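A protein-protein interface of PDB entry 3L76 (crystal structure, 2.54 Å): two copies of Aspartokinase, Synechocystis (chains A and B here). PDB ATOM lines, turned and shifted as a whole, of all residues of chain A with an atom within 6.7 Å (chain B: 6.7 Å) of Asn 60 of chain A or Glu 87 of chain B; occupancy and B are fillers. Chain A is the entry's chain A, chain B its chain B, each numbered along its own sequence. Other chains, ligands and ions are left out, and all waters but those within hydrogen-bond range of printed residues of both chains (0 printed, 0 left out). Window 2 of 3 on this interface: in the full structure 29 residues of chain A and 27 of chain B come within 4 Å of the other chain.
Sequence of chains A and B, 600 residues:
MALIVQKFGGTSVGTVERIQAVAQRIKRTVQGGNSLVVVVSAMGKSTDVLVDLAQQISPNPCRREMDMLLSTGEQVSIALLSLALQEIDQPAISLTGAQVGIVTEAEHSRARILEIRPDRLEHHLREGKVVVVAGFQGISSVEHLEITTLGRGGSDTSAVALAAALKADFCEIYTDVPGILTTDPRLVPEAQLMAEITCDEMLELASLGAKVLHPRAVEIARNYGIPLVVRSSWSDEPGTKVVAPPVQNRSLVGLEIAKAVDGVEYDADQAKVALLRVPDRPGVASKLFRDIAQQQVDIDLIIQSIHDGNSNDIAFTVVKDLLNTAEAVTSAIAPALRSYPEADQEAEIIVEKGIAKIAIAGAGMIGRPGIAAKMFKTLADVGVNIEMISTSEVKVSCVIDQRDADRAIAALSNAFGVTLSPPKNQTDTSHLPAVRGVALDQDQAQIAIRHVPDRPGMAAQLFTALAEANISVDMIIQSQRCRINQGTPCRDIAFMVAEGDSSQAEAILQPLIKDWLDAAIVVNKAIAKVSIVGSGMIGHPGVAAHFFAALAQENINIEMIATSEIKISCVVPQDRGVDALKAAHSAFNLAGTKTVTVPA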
ATOM      1  N   ALA A  54       3.723  18.926  24.185  1.00  0.00           N
ATOM      2  CA  ALA A  54       4.656  18.051  24.880  1.00  0.00           C
ATOM      3  C   ALA A  54       4.079  17.626  26.228  1.00  0.00           C
ATOM      4  O   ALA A  54       4.122  16.449  26.593  1.00  0.00           O
ATOM      5  CB  ALA A  54       6.019  18.738  25.049  1.00  0.00           C
ATOM      6  N   GLN A  55       3.522  18.595  26.951  1.00  0.00           N
ATOM      7  CA  GLN A  55       2.951  18.371  28.280  1.00  0.00           C
ATOM      8  C   GLN A  55       1.931  17.243  28.260  1.00  0.00           C
ATOM      9  O   GLN A  55       1.914  16.389  29.147  1.00  0.00           O
ATOM     10  CB  GLN A  55       2.277  19.648  28.786  1.00  0.00           C
ATOM     11  CG  GLN A  55       2.590  19.999  30.225  1.00  0.00           C
ATOM     12  CD  GLN A  55       4.023  20.453  30.408  1.00  0.00           C
ATOM     13  OE1 GLN A  55       4.960  19.707  30.130  1.00  0.00           O
ATOM     14  NE2 GLN A  55       4.201  21.683  30.883  1.00  0.00           N
ATOM     15  N   ILE A  57       1.794  14.689  26.741  1.00  0.00           N
ATOM     16  CA  ILE A  57       2.366  13.357  26.594  1.00  0.00           C
ATOM     17  C   ILE A  57       3.141  12.955  27.833  1.00  0.00           C
ATOM     18  O   ILE A  57       3.151  11.783  28.212  1.00  0.00           O
ATOM     19  CB  ILE A  57       3.293  13.269  25.368  1.00  0.00           C
ATOM     20  CG1 ILE A  57       2.481  13.351  24.077  1.00  0.00           C
ATOM     21  CG2 ILE A  57       4.082  11.976  25.388  1.00  0.00           C
ATOM     22  CD1 ILE A  57       3.331  13.265  22.844  1.00  0.00           C
ATOM     23  N   SER A  58       3.783  13.940  28.454  1.00  0.00           N
ATOM     24  CA  SER A  58       4.626  13.719  29.624  1.00  0.00           C
ATOM     25  C   SER A  58       4.838  15.031  30.368  1.00  0.00           C
ATOM     26  O   SER A  58       5.481  15.941  29.850  1.00  0.00           O
ATOM     27  CB  SER A  58       5.983  13.153  29.193  1.00  0.00           C
ATOM     28  OG  SER A  58       6.811  12.858  30.303  1.00  0.00           O
ATOM     29  N   PRO A  59       4.279  15.145  31.580  1.00  0.00           N
ATOM     30  CA  PRO A  59       4.575  16.322  32.407  1.00  0.00           C
ATOM     31  C   PRO A  59       5.998  16.281  32.992  1.00  0.00           C
ATOM     32  O   PRO A  59       6.340  17.082  33.859  1.00  0.00           O
ATOM     33  CB  PRO A  59       3.520  16.242  33.515  1.00  0.00           C
ATOM     34  CG  PRO A  59       2.423  15.372  32.944  1.00  0.00           C
ATOM     35  CD  PRO A  59       3.150  14.365  32.112  1.00  0.00           C
ATOM     36  N   ASN A  60       6.809  15.347  32.504  1.00  0.00           N
ATOM     37  CA  ASN A  60       8.212  15.216  32.893  1.00  0.00           C
ATOM     38  C   ASN A  60       9.087  14.961  31.655  1.00  0.00           C
ATOM     39  O   ASN A  60       9.705  13.901  31.521  1.00  0.00           O
ATOM     40  CB  ASN A  60       8.373  14.087  33.919  1.00  0.00           C
ATOM     41  CG  ASN A  60       7.562  12.841  33.556  1.00  0.00           C
ATOM     42  OD1 ASN A  60       6.342  12.906  33.374  1.00  0.00           O
ATOM     43  ND2 ASN A  60       8.239  11.700  33.461  1.00  0.00           N
ATOM     44  N   PRO A  61       9.133  15.945  30.741  1.00  0.00           N
ATOM     45  CA  PRO A  61       9.667  15.805  29.378  1.00  0.00           C
ATOM     46  C   PRO A  61      11.185  15.816  29.290  1.00  0.00           C
ATOM     47  O   PRO A  61      11.767  16.878  29.514  1.00  0.00           O
ATOM     48  CB  PRO A  61       9.133  17.060  28.663  1.00  0.00           C
ATOM     49  CG  PRO A  61       8.127  17.676  29.594  1.00  0.00           C
ATOM     50  CD  PRO A  61       8.572  17.287  30.964  1.00  0.00           C
ATOM     51  N   CYS A  62      11.802  14.683  28.938  1.00  0.00           N
ATOM     52  CA  CYS A  62      13.258  14.622  28.734  1.00  0.00           C
ATOM     53  C   CYS A  62      13.752  15.827  27.917  1.00  0.00           C
ATOM     54  O   CYS A  62      13.260  16.098  26.821  1.00  0.00           O
ATOM     55  CB  CYS A  62      13.679  13.289  28.105  1.00  0.00           C
ATOM     56  SG  CYS A  62      15.035  13.415  26.883  1.00  0.00           S
ATOM     57  N   ARG A  63      14.714  16.556  28.473  1.00  0.00           N
ATOM     58  CA  ARG A  63      15.053  17.881  27.964  1.00  0.00           C
ATOM     59  C   ARG A  63      15.744  17.852  26.604  1.00  0.00           C
ATOM     60  O   ARG A  63      15.666  18.821  25.845  1.00  0.00           O
ATOM     61  CB  ARG A  63      15.887  18.663  28.993  1.00  0.00           C
ATOM     62  N   SER B  82       9.096  10.137  20.357  1.00  0.00           N
ATOM     63  CA  SER B  82      10.122   9.561  21.216  1.00  0.00           C
ATOM     64  C   SER B  82       9.886   9.923  22.689  1.00  0.00           C
ATOM     65  O   SER B  82      10.228   9.143  23.578  1.00  0.00           O
ATOM     66  CB  SER B  82      11.534   9.941  20.741  1.00  0.00           C
ATOM     67  OG  SER B  82      11.960  11.168  21.293  1.00  0.00           O
ATOM     68  N   LEU B  83       9.289  11.091  22.936  1.00  0.00           N
ATOM     69  CA  LEU B  83       8.817  11.451  24.279  1.00  0.00           C
ATOM     70  C   LEU B  83       7.690  10.532  24.722  1.00  0.00           C
ATOM     71  O   LEU B  83       7.674  10.055  25.851  1.00  0.00           O
ATOM     72  CB  LEU B  83       8.307  12.891  24.320  1.00  0.00           C
ATOM     73  CG  LEU B  83       9.355  13.998  24.331  1.00  0.00           C
ATOM     74  CD1 LEU B  83       8.683  15.363  24.242  1.00  0.00           C
ATOM     75  CD2 LEU B  83      10.237  13.884  25.573  1.00  0.00           C
ATOM     76  N   ALA B  84       6.738  10.305  23.823  1.00  0.00           N
ATOM     77  CA  ALA B  84       5.601   9.433  24.083  1.00  0.00           C
ATOM     78  C   ALA B  84       6.047   8.007  24.412  1.00  0.00           C
ATOM     79  O   ALA B  84       5.460   7.344  25.273  1.00  0.00           O
ATOM     80  CB  ALA B  84       4.668   9.437  22.888  1.00  0.00           C
ATOM     81  N   LEU B  85       7.082   7.540  23.715  1.00  0.00           N
ATOM     82  CA  LEU B  85       7.668   6.229  23.976  1.00  0.00           C
ATOM     83  C   LEU B  85       8.312   6.198  25.355  1.00  0.00           C
ATOM     84  O   LEU B  85       8.177   5.220  26.094  1.00  0.00           O
ATOM     85  CB  LEU B  85       8.723   5.895  22.923  1.00  0.00           C
ATOM     86  CG  LEU B  85       8.276   5.390  21.548  1.00  0.00           C
ATOM     87  CD1 LEU B  85       9.361   5.612  20.498  1.00  0.00           C
ATOM     88  CD2 LEU B  85       7.882   3.917  21.614  1.00  0.00           C
ATOM     89  N   GLN B  86       9.017   7.278  25.686  1.00  0.00           N
ATOM     90  CA  GLN B  86       9.723   7.398  26.960  1.00  0.00           C
ATOM     91  C   GLN B  86       8.771   7.483  28.150  1.00  0.00           C
ATOM     92  O   GLN B  86       9.117   7.054  29.248  1.00  0.00           O
ATOM     93  CB  GLN B  86      10.672   8.604  26.942  1.00  0.00           C
ATOM     94  CG  GLN B  86      11.869   8.447  25.994  1.00  0.00           C
ATOM     95  CD  GLN B  86      12.780   9.654  25.992  1.00  0.00           C
ATOM     96  OE1 GLN B  86      13.281  10.060  27.035  1.00  0.00           O
ATOM     97  NE2 GLN B  86      13.001  10.234  24.821  1.00  0.00           N
ATOM     98  N   GLU B  87       7.575   8.024  27.926  1.00  0.00           N
ATOM     99  CA  GLU B  87       6.553   8.079  28.964  1.00  0.00           C
ATOM    100  C   GLU B  87       6.097   6.688  29.359  1.00  0.00           C
ATOM    101  O   GLU B  87       5.842   6.411  30.531  1.00  0.00           O
ATOM    102  CB  GLU B  87       5.342   8.898  28.520  1.00  0.00           C
ATOM    103  CG  GLU B  87       5.084  10.121  29.394  1.00  0.00           C
ATOM    104  CD  GLU B  87       5.221   9.843  30.885  1.00  0.00           C
ATOM    105  OE1 GLU B  87       4.656   8.839  31.367  1.00  0.00           O
ATOM    106  OE2 GLU B  87       5.889  10.638  31.578  1.00  0.00           O
ATOM    107  N   ILE B  88       5.982   5.813  28.378  1.00  0.00           N
ATOM    108  CA  ILE B  88       5.559   4.452  28.657  1.00  0.00           C
ATOM    109  C   ILE B  88       6.779   3.543  28.777  1.00  0.00           C
ATOM    110  O   ILE B  88       6.725   2.343  28.493  1.00  0.00           O
ATOM    111  CB  ILE B  88       4.569   3.930  27.605  1.00  0.00           C
ATOM    112  CG1 ILE B  88       5.218   3.910  26.216  1.00  0.00           C
ATOM    113  CG2 ILE B  88       3.315   4.787  27.603  1.00  0.00           C
ATOM    114  CD1 ILE B  88       4.355   3.267  25.163  1.00  0.00           C
ATOM    115  N   ASP B  89       7.883   4.138  29.202  1.00  0.00           N
ATOM    116  CA  ASP B  89       9.078   3.379  29.552  1.00  0.00           C
ATOM    117  C   ASP B  89       9.600   2.546  28.385  1.00  0.00           C
ATOM    118  O   ASP B  89       9.941   1.370  28.542  1.00  0.00           O
ATOM    119  CB  ASP B  89       8.804   2.499  30.772  1.00  0.00           C
ATOM    120  CG  ASP B  89       8.153   3.271  31.906  1.00  0.00           C
ATOM    121  OD1 ASP B  89       8.825   4.158  32.491  1.00  0.00           O
ATOM    122  OD2 ASP B  89       6.966   2.993  32.202  1.00  0.00           O
ATOM    123  N   GLN B  90       9.657   3.171  27.214  1.00  0.00           N
ATOM    124  CA  GLN B  90      10.316   2.577  26.062  1.00  0.00           C
ATOM    125  C   GLN B  90      11.513   3.419  25.676  1.00  0.00           C
ATOM    126  O   GLN B  90      11.357   4.510  25.125  1.00  0.00           O
ATOM    127  CB  GLN B  90       9.359   2.476  24.866  1.00  0.00           C
ATOM    128  CG  GLN B  90       9.171   1.059  24.322  1.00  0.00           C
ATOM    129  CD  GLN B  90      10.478   0.359  23.951  1.00  0.00           C
ATOM    130  OE1 GLN B  90      10.561  -0.868  23.974  1.00  0.00           O
ATOM    131  NE2 GLN B  90      11.496   1.135  23.617  1.00  0.00           N
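Among the printed residues, merely in contact across the chains: Ile 57 of chain A with Glu 87 of chain B, Ile 57 of chain A with Ala 84 of chain B, Cys 62 of chain A with Leu 83 of chain B and Ile 57 of chain A with Leu 83 of chain B.
OG of Ser 58 of chain A sits at hydrogen-bond distance from OD1 of Asn 60 of chain A (3.1 Å).
The side-chain amide nitrogen (NE2) of Gln 86 of chain B sits close to the backbone carbonyl oxygen (O) of Ser 82 of chain B (3.2 Å).
Of the printed residues of chain B, Asn 60 of chain A touches Glu 87.
Glu 87 of chain B touches just these residues of chain A: Ile 57 (2.8 Å), Ser 58 (2.7 Å) and Asn 60 (2.9 Å).
Of the printed residues of chain A, Gln 86 of chain B touches Cys 62.
Of the printed residues of chain A, Leu 83 of chain B touches Ile 57 (3.9 Å) and Cys 62 (3.8 Å).
Of the printed residues of chain B, Ile 57 of chain A touches Leu 83, Ala 84 and Glu 87.
Of the printed residues of chain B, Cys 62 of chain A touches Leu 83 and Gln 86.
Printed residues of chain A within 4 Å of Ala 84 of chain B: Ile 57 (3.2 Å).
The nearest residue of chain B that does not touch Asn 60 of chain A is Leu 83 of chain B (6.0 Å).
The nearest printed residue of chain B that does not touch Cys 62 of chain A is Ser 82 of chain B (6.8 Å).
No position is printed for both chains.
Of the 7 pairs that touch across the chains among the printed residues, none has its exchanged pair printed and touching as well.
Hydrophobic or aromatic side chains of chain B that line the printed part of chain A: Leu 83 and Ala 84.
Of the 9 printed residues of chain A, 4 touch a printed residue of chain B.
Among the printed residues, 7 pairs touch across the chains.
Among the printed residues, no Asp or Glu carboxylate lies within 4 Å of a Lys or Arg side-chain nitrogen of the other chain.
The side-chain hydroxyl of Ser 58 of chain A sits at hydrogen-bond distance from the side-chain carboxylate of Glu 87 of chain B.
The side-chain carboxylate (OE2) of Glu 87 of chain B sits close to the side-chain amide oxygen (OD1) of Asn 60 of chain A (2.9 Å).
SG of Cys 62 of chain A lies close to OE1 of Gln 86 of chain B, at 3.8 Å.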
